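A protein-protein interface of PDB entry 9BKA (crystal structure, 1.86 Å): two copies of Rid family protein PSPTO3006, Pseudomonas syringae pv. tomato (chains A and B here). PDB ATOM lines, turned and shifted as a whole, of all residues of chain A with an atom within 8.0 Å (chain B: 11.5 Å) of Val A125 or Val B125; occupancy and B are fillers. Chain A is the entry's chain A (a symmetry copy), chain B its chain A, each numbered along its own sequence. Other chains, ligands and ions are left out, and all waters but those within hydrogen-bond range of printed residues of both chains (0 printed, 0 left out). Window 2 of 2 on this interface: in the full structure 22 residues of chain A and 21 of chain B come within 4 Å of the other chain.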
ATOM      1  N   PHE A  84     -23.687  -0.222 -21.347  1.00  0.00           N
ATOM      2  CA  PHE A  84     -24.502  -0.250 -20.143  1.00  0.00           C
ATOM      3  C   PHE A  84     -25.755   0.563 -20.417  1.00  0.00           C
ATOM      4  O   PHE A  84     -25.664   1.760 -20.704  1.00  0.00           O
ATOM      5  CB  PHE A  84     -23.751   0.333 -18.944  1.00  0.00           C
ATOM      6  CG  PHE A  84     -22.426  -0.339 -18.654  1.00  0.00           C
ATOM      7  CD1 PHE A  84     -22.379  -1.564 -18.007  1.00  0.00           C
ATOM      8  CD2 PHE A  84     -21.230   0.273 -18.995  1.00  0.00           C
ATOM      9  CE1 PHE A  84     -21.153  -2.175 -17.717  1.00  0.00           C
ATOM     10  CE2 PHE A  84     -20.008  -0.334 -18.725  1.00  0.00           C
ATOM     11  CZ  PHE A  84     -19.967  -1.545 -18.071  1.00  0.00           C
ATOM     12  N   LEU A  85     -26.909  -0.086 -20.327  1.00  0.00           N
ATOM     13  CA  LEU A  85     -28.213   0.535 -20.546  1.00  0.00           C
ATOM     14  C   LEU A  85     -28.982   0.657 -19.236  1.00  0.00           C
ATOM     15  O   LEU A  85     -28.837  -0.166 -18.331  1.00  0.00           O
ATOM     16  CB  LEU A  85     -29.054  -0.297 -21.529  1.00  0.00           C
ATOM     17  CG  LEU A  85     -28.468  -0.473 -22.926  1.00  0.00           C
ATOM     18  CD1 LEU A  85     -29.453  -1.256 -23.796  1.00  0.00           C
ATOM     19  CD2 LEU A  85     -28.204   0.891 -23.536  1.00  0.00           C
ATOM     20  N   VAL A  86     -29.835   1.674 -19.155  1.00  0.00           N
ATOM     21  CA  VAL A  86     -30.808   1.771 -18.080  1.00  0.00           C
ATOM     22  C   VAL A  86     -32.201   1.623 -18.689  1.00  0.00           C
ATOM     23  O   VAL A  86     -32.411   1.805 -19.894  1.00  0.00           O
ATOM     24  CB  VAL A  86     -30.667   3.088 -17.283  1.00  0.00           C
ATOM     25  CG1 VAL A  86     -29.220   3.294 -16.855  1.00  0.00           C
ATOM     26  CG2 VAL A  86     -31.101   4.229 -18.094  1.00  0.00           C
ATOM     27  N   GLY A  87     -33.160   1.271 -17.844  1.00  0.00           N
ATOM     28  CA  GLY A  87     -34.489   0.976 -18.337  1.00  0.00           C
ATOM     29  C   GLY A  87     -35.161   2.193 -18.945  1.00  0.00           C
ATOM     30  O   GLY A  87     -34.939   3.331 -18.535  1.00  0.00           O
ATOM     31  N   GLY A  93     -39.425  -0.160 -18.372  1.00  0.00           N
ATOM     32  CA  GLY A  93     -38.387  -0.235 -17.367  1.00  0.00           C
ATOM     33  C   GLY A  93     -37.336  -1.293 -17.624  1.00  0.00           C
ATOM     34  O   GLY A  93     -36.352  -1.365 -16.874  1.00  0.00           O
ATOM     35  N   LYS A  94     -37.511  -2.111 -18.656  1.00  0.00           N
ATOM     36  CA  LYS A  94     -36.435  -2.953 -19.160  1.00  0.00           C
ATOM     37  C   LYS A  94     -35.568  -2.147 -20.118  1.00  0.00           C
ATOM     38  O   LYS A  94     -35.997  -1.131 -20.669  1.00  0.00           O
ATOM     39  CB  LYS A  94     -36.987  -4.172 -19.892  1.00  0.00           C
ATOM     40  CG  LYS A  94     -37.956  -5.033 -19.087  1.00  0.00           C
ATOM     41  CD  LYS A  94     -38.605  -6.067 -20.004  1.00  0.00           C
ATOM     42  CE  LYS A  94     -39.437  -7.084 -19.221  1.00  0.00           C
ATOM     43  NZ  LYS A  94     -39.219  -6.991 -17.755  1.00  0.00           N
ATOM     44  N   LEU A  95     -34.340  -2.619 -20.325  1.00  0.00           N
ATOM     45  CA  LEU A  95     -33.479  -2.001 -21.323  1.00  0.00           C
ATOM     46  C   LEU A  95     -34.175  -2.028 -22.678  1.00  0.00           C
ATOM     47  O   LEU A  95     -34.942  -2.947 -22.986  1.00  0.00           O
ATOM     48  CB  LEU A  95     -32.116  -2.710 -21.387  1.00  0.00           C
ATOM     49  CG  LEU A  95     -31.983  -4.102 -22.016  1.00  0.00           C
ATOM     50  CD1 LEU A  95     -30.513  -4.513 -22.049  1.00  0.00           C
ATOM     51  CD2 LEU A  95     -32.822  -5.163 -21.334  1.00  0.00           C
ATOM     52  N   LEU A 122     -25.755  -4.867 -21.400  1.00  0.00           N
ATOM     53  CA  LEU A 122     -26.572  -5.295 -20.268  1.00  0.00           C
ATOM     54  C   LEU A 122     -27.215  -4.086 -19.604  1.00  0.00           C
ATOM     55  O   LEU A 122     -26.833  -2.940 -19.845  1.00  0.00           O
ATOM     56  CB  LEU A 122     -25.743  -6.081 -19.251  1.00  0.00           C
ATOM     57  CG  LEU A 122     -24.451  -5.402 -18.811  1.00  0.00           C
ATOM     58  CD1 LEU A 122     -24.619  -4.698 -17.491  1.00  0.00           C
ATOM     59  CD2 LEU A 122     -23.361  -6.441 -18.731  1.00  0.00           C
ATOM     60  N   GLN A 123     -28.173  -4.362 -18.728  1.00  0.00           N
ATOM     61  CA  GLN A 123     -28.910  -3.317 -18.030  1.00  0.00           C
ATOM     62  C   GLN A 123     -28.370  -3.124 -16.623  1.00  0.00           C
ATOM     63  O   GLN A 123     -28.281  -4.085 -15.854  1.00  0.00           O
ATOM     64  CB  GLN A 123     -30.408  -3.647 -17.965  1.00  0.00           C
ATOM     65  CG  GLN A 123     -31.249  -2.474 -17.423  1.00  0.00           C
ATOM     66  CD  GLN A 123     -32.746  -2.763 -17.435  1.00  0.00           C
ATOM     67  OE1 GLN A 123     -33.192  -3.720 -18.059  1.00  0.00           O
ATOM     68  NE2 GLN A 123     -33.519  -1.950 -16.711  1.00  0.00           N
ATOM     69  N   VAL A 124     -28.030  -1.879 -16.287  1.00  0.00           N
ATOM     70  CA  VAL A 124     -27.599  -1.519 -14.942  1.00  0.00           C
ATOM     71  C   VAL A 124     -28.676  -0.667 -14.283  1.00  0.00           C
ATOM     72  O   VAL A 124     -29.721  -0.381 -14.889  1.00  0.00           O
ATOM     73  CB  VAL A 124     -26.243  -0.785 -14.953  1.00  0.00           C
ATOM     74  CG1 VAL A 124     -25.181  -1.649 -15.611  1.00  0.00           C
ATOM     75  CG2 VAL A 124     -26.373   0.538 -15.677  1.00  0.00           C
ATOM     76  N   VAL A 125     -28.429  -0.257 -13.034  1.00  0.00           N
ATOM     77  CA  VAL A 125     -29.435   0.491 -12.282  1.00  0.00           C
ATOM     78  C   VAL A 125     -29.474   1.942 -12.726  1.00  0.00           C
ATOM     79  O   VAL A 125     -30.549   2.505 -12.973  1.00  0.00           O
ATOM     80  CB  VAL A 125     -29.170   0.383 -10.768  1.00  0.00           C
ATOM     81  CG1 VAL A 125     -30.105   1.308 -10.014  1.00  0.00           C
ATOM     82  CG2 VAL A 125     -29.353  -1.068 -10.300  1.00  0.00           C
ATOM     83  N   ALA A 126     -28.307   2.569 -12.834  1.00  0.00           N
ATOM     84  CA  ALA A 126     -28.247   4.007 -13.038  1.00  0.00           C
ATOM     85  C   ALA A 126     -26.876   4.360 -13.569  1.00  0.00           C
ATOM     86  O   ALA A 126     -25.898   3.654 -13.314  1.00  0.00           O
ATOM     87  CB  ALA A 126     -28.527   4.775 -11.735  1.00  0.00           C
ATOM     88  N   LEU A 127     -26.823   5.456 -14.294  1.00  0.00           N
ATOM     89  CA  LEU A 127     -25.616   6.053 -14.833  1.00  0.00           C
ATOM     90  C   LEU A 127     -25.362   7.373 -14.118  1.00  0.00           C
ATOM     91  O   LEU A 127     -26.302   7.973 -13.585  1.00  0.00           O
ATOM     92  CB  LEU A 127     -25.755   6.274 -16.348  1.00  0.00           C
ATOM     93  CG  LEU A 127     -26.007   4.966 -17.119  1.00  0.00           C
ATOM     94  CD1 LEU A 127     -26.228   5.218 -18.599  1.00  0.00           C
ATOM     95  CD2 LEU A 127     -24.863   3.980 -16.931  1.00  0.00           C
ATOM     96  N   ALA A 132     -29.344  10.134 -18.938  1.00  0.00           N
ATOM     97  CA  ALA A 132     -28.638   9.224 -19.830  1.00  0.00           C
ATOM     98  C   ALA A 132     -29.224   7.816 -19.737  1.00  0.00           C
ATOM     99  O   ALA A 132     -29.463   7.302 -18.642  1.00  0.00           O
ATOM    100  CB  ALA A 132     -27.150   9.217 -19.488  1.00  0.00           C
ATOM    101  N   LEU B  34     -23.735 -16.024 -23.284  1.00  0.00           N
ATOM    102  CA  LEU B  34     -24.957 -16.415 -22.616  1.00  0.00           C
ATOM    103  C   LEU B  34     -25.143 -17.932 -22.702  1.00  0.00           C
ATOM    104  O   LEU B  34     -24.577 -18.582 -23.588  1.00  0.00           O
ATOM    105  CB  LEU B  34     -26.137 -15.683 -23.276  1.00  0.00           C
ATOM    106  CG  LEU B  34     -26.189 -14.179 -23.032  1.00  0.00           C
ATOM    107  CD1 LEU B  34     -26.988 -13.504 -24.140  1.00  0.00           C
ATOM    108  CD2 LEU B  34     -26.810 -13.891 -21.666  1.00  0.00           C
ATOM    109  N   PRO B  47     -36.315 -19.044 -17.345  1.00  0.00           N
ATOM    110  CA  PRO B  47     -35.151 -19.647 -16.683  1.00  0.00           C
ATOM    111  C   PRO B  47     -35.151 -21.165 -16.778  1.00  0.00           C
ATOM    112  O   PRO B  47     -34.082 -21.760 -16.916  1.00  0.00           O
ATOM    113  CB  PRO B  47     -35.274 -19.157 -15.232  1.00  0.00           C
ATOM    114  CG  PRO B  47     -36.063 -17.880 -15.323  1.00  0.00           C
ATOM    115  CD  PRO B  47     -37.027 -18.087 -16.474  1.00  0.00           C
ATOM    116  N   VAL B  83     -18.285 -11.554 -14.749  1.00  0.00           N
ATOM    117  CA  VAL B  83     -19.512 -12.333 -14.604  1.00  0.00           C
ATOM    118  C   VAL B  83     -20.629 -11.398 -14.174  1.00  0.00           C
ATOM    119  O   VAL B  83     -20.540 -10.777 -13.113  1.00  0.00           O
ATOM    120  CB  VAL B  83     -19.358 -13.463 -13.575  1.00  0.00           C
ATOM    121  CG1 VAL B  83     -20.710 -14.213 -13.405  1.00  0.00           C
ATOM    122  CG2 VAL B  83     -18.257 -14.401 -13.992  1.00  0.00           C
ATOM    123  N   PHE B  84     -21.690 -11.316 -14.980  1.00  0.00           N
ATOM    124  CA  PHE B  84     -22.857 -10.507 -14.666  1.00  0.00           C
ATOM    125  C   PHE B  84     -24.000 -11.456 -14.348  1.00  0.00           C
ATOM    126  O   PHE B  84     -24.395 -12.256 -15.202  1.00  0.00           O
ATOM    127  CB  PHE B  84     -23.241  -9.598 -15.835  1.00  0.00           C
ATOM    128  CG  PHE B  84     -22.126  -8.686 -16.305  1.00  0.00           C
ATOM    129  CD1 PHE B  84     -21.806  -7.537 -15.597  1.00  0.00           C
ATOM    130  CD2 PHE B  84     -21.428  -8.960 -17.470  1.00  0.00           C
ATOM    131  CE1 PHE B  84     -20.792  -6.682 -16.045  1.00  0.00           C
ATOM    132  CE2 PHE B  84     -20.410  -8.124 -17.912  1.00  0.00           C
ATOM    133  CZ  PHE B  84     -20.103  -6.977 -17.213  1.00  0.00           C
ATOM    134  N   LEU B  85     -24.522 -11.363 -13.132  1.00  0.00           N
ATOM    135  CA  LEU B  85     -25.631 -12.185 -12.655  1.00  0.00           C
ATOM    136  C   LEU B  85     -26.897 -11.351 -12.501  1.00  0.00           C
ATOM    137  O   LEU B  85     -26.842 -10.156 -12.201  1.00  0.00           O
ATOM    138  CB  LEU B  85     -25.295 -12.816 -11.294  1.00  0.00           C
ATOM    139  CG  LEU B  85     -24.085 -13.745 -11.269  1.00  0.00           C
ATOM    140  CD1 LEU B  85     -23.931 -14.344  -9.869  1.00  0.00           C
ATOM    141  CD2 LEU B  85     -24.279 -14.850 -12.290  1.00  0.00           C
ATOM    142  N   VAL B  86     -28.045 -11.998 -12.672  1.00  0.00           N
ATOM    143  CA  VAL B  86     -29.320 -11.400 -12.313  1.00  0.00           C
ATOM    144  C   VAL B  86     -29.905 -12.196 -11.146  1.00  0.00           C
ATOM    145  O   VAL B  86     -29.527 -13.344 -10.884  1.00  0.00           O
ATOM    146  CB  VAL B  86     -30.293 -11.340 -13.512  1.00  0.00           C
ATOM    147  CG1 VAL B  86     -29.609 -10.710 -14.717  1.00  0.00           C
ATOM    148  CG2 VAL B  86     -30.758 -12.686 -13.865  1.00  0.00           C
ATOM    149  N   GLY B  87     -30.826 -11.567 -10.430  1.00  0.00           N
ATOM    150  CA  GLY B  87     -31.351 -12.178  -9.226  1.00  0.00           C
ATOM    151  C   GLY B  87     -32.123 -13.451  -9.516  1.00  0.00           C
ATOM    152  O   GLY B  87     -32.752 -13.607 -10.562  1.00  0.00           O
ATOM    153  N   ALA B  88     -32.060 -14.378  -8.566  1.00  0.00           N
ATOM    154  CA  ALA B  88     -32.647 -15.702  -8.697  1.00  0.00           C
ATOM    155  C   ALA B  88     -33.685 -15.929  -7.603  1.00  0.00           C
ATOM    156  O   ALA B  88     -33.559 -15.407  -6.491  1.00  0.00           O
ATOM    157  CB  ALA B  88     -31.577 -16.799  -8.602  1.00  0.00           C
ATOM    158  N   GLU B  89     -34.684 -16.757  -7.917  1.00  0.00           N
ATOM    159  CA  GLU B  89     -35.729 -17.062  -6.939  1.00  0.00           C
ATOM    160  C   GLU B  89     -35.179 -17.799  -5.713  1.00  0.00           C
ATOM    161  O   GLU B  89     -35.672 -17.585  -4.595  1.00  0.00           O
ATOM    162  CB  GLU B  89     -36.844 -17.876  -7.614  1.00  0.00           C
ATOM    163  CG  GLU B  89     -36.416 -19.252  -8.121  1.00  0.00           C
ATOM    164  CD  GLU B  89     -37.550 -20.009  -8.799  1.00  0.00           C
ATOM    165  OE1 GLU B  89     -38.607 -19.399  -9.051  1.00  0.00           O
ATOM    166  OE2 GLU B  89     -37.379 -21.218  -9.078  1.00  0.00           O
ATOM    167  N   GLY B  93     -34.195 -12.928  -5.104  1.00  0.00           N
ATOM    168  CA  GLY B  93     -33.947 -11.784  -5.955  1.00  0.00           C
ATOM    169  C   GLY B  93     -32.551 -11.213  -5.851  1.00  0.00           C
ATOM    170  O   GLY B  93     -32.212 -10.298  -6.617  1.00  0.00           O
ATOM    171  N   LYS B  94     -31.733 -11.719  -4.936  1.00  0.00           N
ATOM    172  CA  LYS B  94     -30.302 -11.452  -4.952  1.00  0.00           C
ATOM    173  C   LYS B  94     -29.616 -12.420  -5.906  1.00  0.00           C
ATOM    174  O   LYS B  94     -30.146 -13.485  -6.228  1.00  0.00           O
ATOM    175  CB  LYS B  94     -29.698 -11.612  -3.560  1.00  0.00           C
ATOM    176  CG  LYS B  94     -30.348 -10.771  -2.467  1.00  0.00           C
ATOM    177  CD  LYS B  94     -29.809 -11.199  -1.104  1.00  0.00           C
ATOM    178  CE  LYS B  94     -30.274 -10.265   0.014  1.00  0.00           C
ATOM    179  NZ  LYS B  94     -30.918  -9.032  -0.505  1.00  0.00           N
ATOM    180  N   LEU B  95     -28.417 -12.045  -6.350  1.00  0.00           N
ATOM    181  CA  LEU B  95     -27.620 -12.957  -7.159  1.00  0.00           C
ATOM    182  C   LEU B  95     -27.400 -14.255  -6.389  1.00  0.00           C
ATOM    183  O   LEU B  95     -27.312 -14.261  -5.157  1.00  0.00           O
ATOM    184  CB  LEU B  95     -26.281 -12.313  -7.552  1.00  0.00           C
ATOM    185  CG  LEU B  95     -25.165 -12.125  -6.518  1.00  0.00           C
ATOM    186  CD1 LEU B  95     -23.917 -11.573  -7.203  1.00  0.00           C
ATOM    187  CD2 LEU B  95     -25.562 -11.256  -5.344  1.00  0.00           C
ATOM    188  N   ALA B 121     -17.301 -10.271 -10.381  1.00  0.00           N
ATOM    189  CA  ALA B 121     -18.645 -10.835 -10.422  1.00  0.00           C
ATOM    190  C   ALA B 121     -19.595  -9.909  -9.682  1.00  0.00           C
ATOM    191  O   ALA B 121     -19.263  -9.431  -8.591  1.00  0.00           O
ATOM    192  CB  ALA B 121     -18.675 -12.241  -9.807  1.00  0.00           C
ATOM    193  N   LEU B 122     -20.758  -9.631 -10.275  1.00  0.00           N
ATOM    194  CA  LEU B 122     -21.688  -8.688  -9.658  1.00  0.00           C
ATOM    195  C   LEU B 122     -23.085  -8.890 -10.227  1.00  0.00           C
ATOM    196  O   LEU B 122     -23.274  -9.550 -11.250  1.00  0.00           O
ATOM    197  CB  LEU B 122     -21.232  -7.242  -9.867  1.00  0.00           C
ATOM    198  CG  LEU B 122     -20.901  -6.873 -11.306  1.00  0.00           C
ATOM    199  CD1 LEU B 122     -22.047  -6.158 -11.972  1.00  0.00           C
ATOM    200  CD2 LEU B 122     -19.658  -6.018 -11.313  1.00  0.00           C
ATOM    201  N   GLN B 123     -24.059  -8.272  -9.573  1.00  0.00           N
ATOM    202  CA  GLN B 123     -25.457  -8.390  -9.969  1.00  0.00           C
ATOM    203  C   GLN B 123     -25.895  -7.170 -10.761  1.00  0.00           C
ATOM    204  O   GLN B 123     -25.741  -6.037 -10.297  1.00  0.00           O
ATOM    205  CB  GLN B 123     -26.366  -8.561  -8.743  1.00  0.00           C
ATOM    206  CG  GLN B 123     -27.819  -8.898  -9.129  1.00  0.00           C
ATOM    207  CD  GLN B 123     -28.711  -9.153  -7.919  1.00  0.00           C
ATOM    208  OE1 GLN B 123     -28.219  -9.323  -6.807  1.00  0.00           O
ATOM    209  NE2 GLN B 123     -30.028  -9.145  -8.131  1.00  0.00           N
ATOM    210  N   VAL B 124     -26.459  -7.409 -11.946  1.00  0.00           N
ATOM    211  CA  VAL B 124     -27.027  -6.350 -12.774  1.00  0.00           C
ATOM    212  C   VAL B 124     -28.543  -6.494 -12.797  1.00  0.00           C
ATOM    213  O   VAL B 124     -29.106  -7.409 -12.173  1.00  0.00           O
ATOM    214  CB  VAL B 124     -26.449  -6.368 -14.203  1.00  0.00           C
ATOM    215  CG1 VAL B 124     -24.937  -6.222 -14.161  1.00  0.00           C
ATOM    216  CG2 VAL B 124     -26.838  -7.650 -14.907  1.00  0.00           C
ATOM    217  N   VAL B 125     -29.216  -5.589 -13.516  1.00  0.00           N
ATOM    218  CA  VAL B 125     -30.677  -5.586 -13.532  1.00  0.00           C
ATOM    219  C   VAL B 125     -31.210  -6.672 -14.447  1.00  0.00           C
ATOM    220  O   VAL B 125     -32.116  -7.431 -14.076  1.00  0.00           O
ATOM    221  CB  VAL B 125     -31.211  -4.201 -13.948  1.00  0.00           C
ATOM    222  CG1 VAL B 125     -32.714  -4.264 -14.139  1.00  0.00           C
ATOM    223  CG2 VAL B 125     -30.846  -3.151 -12.890  1.00  0.00           C
ATOM    224  N   ALA B 126     -30.660  -6.768 -15.652  1.00  0.00           N
ATOM    225  CA  ALA B 126     -31.239  -7.622 -16.673  1.00  0.00           C
ATOM    226  C   ALA B 126     -30.193  -7.884 -17.733  1.00  0.00           C
ATOM    227  O   ALA B 126     -29.285  -7.074 -17.938  1.00  0.00           O
ATOM    228  CB  ALA B 126     -32.488  -6.982 -17.307  1.00  0.00           C
ATOM    229  N   LEU B 127     -30.339  -9.008 -18.399  1.00  0.00           N
ATOM    230  CA  LEU B 127     -29.524  -9.438 -19.519  1.00  0.00           C
ATOM    231  C   LEU B 127     -30.380  -9.419 -20.780  1.00  0.00           C
ATOM    232  O   LEU B 127     -31.609  -9.509 -20.688  1.00  0.00           O
ATOM    233  CB  LEU B 127     -28.960 -10.844 -19.267  1.00  0.00           C
ATOM    234  CG  LEU B 127     -28.083 -10.916 -18.006  1.00  0.00           C
ATOM    235  CD1 LEU B 127     -27.607 -12.329 -17.728  1.00  0.00           C
ATOM    236  CD2 LEU B 127     -26.884  -9.983 -18.108  1.00  0.00           C
ATOM    237  N   PRO B 128     -29.793  -9.254 -21.967  1.00  0.00           N
ATOM    238  CA  PRO B 128     -30.645  -9.097 -23.159  1.00  0.00           C
ATOM    239  C   PRO B 128     -31.441 -10.354 -23.519  1.00  0.00           C
ATOM    240  O   PRO B 128     -32.473 -10.246 -24.195  1.00  0.00           O
ATOM    241  CB  PRO B 128     -29.658  -8.703 -24.268  1.00  0.00           C
ATOM    242  CG  PRO B 128     -28.312  -8.884 -23.739  1.00  0.00           C
ATOM    243  CD  PRO B 128     -28.371  -8.965 -22.241  1.00  0.00           C
ATOM    244  N   LEU B 129     -31.023 -11.520 -23.053  1.00  0.00           N
ATOM    245  CA  LEU B 129     -31.676 -12.783 -23.382  1.00  0.00           C
ATOM    246  C   LEU B 129     -32.680 -13.145 -22.287  1.00  0.00           C
ATOM    247  O   LEU B 129     -32.278 -13.299 -21.123  1.00  0.00           O
ATOM    248  CB  LEU B 129     -30.625 -13.883 -23.528  1.00  0.00           C
ATOM    249  CG  LEU B 129     -31.035 -15.316 -23.867  1.00  0.00           C
ATOM    250  CD1 LEU B 129     -31.821 -15.329 -25.163  1.00  0.00           C
ATOM    251  CD2 LEU B 129     -29.813 -16.235 -23.959  1.00  0.00           C
ATOM    252  N   PRO B 130     -33.974 -13.273 -22.601  1.00  0.00           N
ATOM    253  CA  PRO B 130     -34.944 -13.672 -21.573  1.00  0.00           C
ATOM    254  C   PRO B 130     -34.620 -15.047 -21.012  1.00  0.00           C
ATOM    255  O   PRO B 130     -34.306 -15.978 -21.752  1.00  0.00           O
ATOM    256  CB  PRO B 130     -36.281 -13.687 -22.331  1.00  0.00           C
ATOM    257  CG  PRO B 130     -36.062 -12.853 -23.512  1.00  0.00           C
ATOM    258  CD  PRO B 130     -34.625 -13.015 -23.896  1.00  0.00           C
ATOM    259  N   GLY B 131     -34.704 -15.170 -19.693  1.00  0.00           N
ATOM    260  CA  GLY B 131     -34.442 -16.429 -19.020  1.00  0.00           C
ATOM    261  C   GLY B 131     -33.009 -16.609 -18.554  1.00  0.00           C
ATOM    262  O   GLY B 131     -32.745 -17.475 -17.705  1.00  0.00           O
ATOM    263  N   ALA B 132     -32.085 -15.813 -19.073  1.00  0.00           N
ATOM    264  CA  ALA B 132     -30.680 -15.932 -18.711  1.00  0.00           C
ATOM    265  C   ALA B 132     -30.423 -15.319 -17.335  1.00  0.00           C
ATOM    266  O   ALA B 132     -30.890 -14.217 -17.037  1.00  0.00           O
ATOM    267  CB  ALA B 132     -29.814 -15.259 -19.774  1.00  0.00           C
ATOM    268  N   LEU B 133     -29.668 -16.037 -16.501  1.00  0.00           N
ATOM    269  CA  LEU B 133     -29.283 -15.562 -15.183  1.00  0.00           C
ATOM    270  C   LEU B 133     -27.821 -15.153 -15.108  1.00  0.00           C
ATOM    271  O   LEU B 133     -27.421 -14.539 -14.114  1.00  0.00           O
ATOM    272  CB  LEU B 133     -29.562 -16.635 -14.119  1.00  0.00           C
ATOM    273  CG  LEU B 133     -31.030 -17.038 -13.920  1.00  0.00           C
ATOM    274  CD1 LEU B 133     -31.122 -18.290 -13.049  1.00  0.00           C
ATOM    275  CD2 LEU B 133     -31.835 -15.918 -13.282  1.00  0.00           C
ATOM    276  N   ILE B 134     -27.035 -15.429 -16.142  1.00  0.00           N
ATOM    277  CA  ILE B 134     -25.606 -15.127 -16.139  1.00  0.00           C
ATOM    278  C   ILE B 134     -25.190 -14.787 -17.560  1.00  0.00           C
ATOM    279  O   ILE B 134     -25.706 -15.358 -18.530  1.00  0.00           O
ATOM    280  CB  ILE B 134     -24.794 -16.313 -15.558  1.00  0.00           C
ATOM    281  CG1 ILE B 134     -23.292 -16.076 -15.624  1.00  0.00           C
ATOM    282  CG2 ILE B 134     -25.153 -17.650 -16.267  1.00  0.00           C
ATOM    283  CD1 ILE B 134     -22.505 -17.209 -14.952  1.00  0.00           C
ATOM    284  N   GLU B 135     -24.285 -13.818 -17.678  1.00  0.00           N
ATOM    285  CA  GLU B 135     -23.554 -13.547 -18.910  1.00  0.00           C
ATOM    286  C   GLU B 135     -22.090 -13.355 -18.542  1.00  0.00           C
ATOM    287  O   GLU B 135     -21.785 -12.697 -17.544  1.00  0.00           O
ATOM    288  CB  GLU B 135     -24.089 -12.291 -19.616  1.00  0.00           C
ATOM    289  CG  GLU B 135     -23.361 -11.965 -20.905  1.00  0.00           C
ATOM    290  CD  GLU B 135     -24.101 -10.967 -21.772  1.00  0.00           C
ATOM    291  OE1 GLU B 135     -25.207 -10.546 -21.400  1.00  0.00           O
ATOM    292  OE2 GLU B 135     -23.575 -10.618 -22.847  1.00  0.00           O
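The backbone NH (N) of Val B125 is in hydrogen-bond range of the backbone carbonyl oxygen (O) of Gln A123 (2.9 Å). The backbone NH (N) of Gln A123 lies within hydrogen-bond range of the backbone carbonyl oxygen (O) of Ala B126.
O of Glu B135 sits at hydrogen-bond distance from N of Phe B84, at 2.9 Å. N of Val B124 sits at hydrogen-bond distance from O of Leu B85 (2.8 Å). The backbone NH (N) of Leu A85 sits at hydrogen-bond distance from the backbone carbonyl oxygen (O) of Leu A122 (2.9 Å). The backbone NH (N) of Val A124 is in hydrogen-bond range of the backbone carbonyl oxygen (O) of Leu A85 (2.8 Å). NE2 of Gln A123 sits close to N of Gly A87, 3.4 Å away. N of Leu A95 sits at hydrogen-bond distance from OE1 of Gln A123 (2.8 Å).
Among the printed residues, pairs that only touch across the chains: Leu A122 with Phe B84, Leu A122 with Val B124, Leu A122 with Ala B126, Gln A123 with Val B124, Val A124 with Val B125 and Val A125 with Val B125.
No residue of chain B comes within 4 Å of Val A86. No residue of chain B comes within 4 Å of Ala A126. Printed residues of chain A within 4 Å of Phe B84: Leu A122. Printed residues of chain A within 4 Å of Val B124: Leu A122 (3.7 Å) and Gln A123 (3.4 Å). Val B125 touches three residues of chain A. Of the printed residues of chain A, Ala B126 touches Leu A122 (3.9 Å) and Gln A123 (3.0 Å). The nearest printed residue of chain A that does not touch Phe B84 is Phe A84 (4.8 Å).
Printed residues of chain A that touch a printed residue of chain B: Leu A122, Gln A123, Val A124 and Val A125. Among the printed residues, 8 pairs touch across the chains.
Leu A122 touches Phe B84, but with the chains exchanged Phe A84 does not touch Leu B122 (7.0 Å). Leu A122 touches Val B124, but with the chains exchanged Val A124 does not touch Leu B122 (6.6 Å). Gln A123 touches Ala B126, but with the chains exchanged Ala A126 does not touch Gln B123 (9.3 Å). Val B125 touches its own counterpart, Val A125. 14 positions are printed for both chains.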
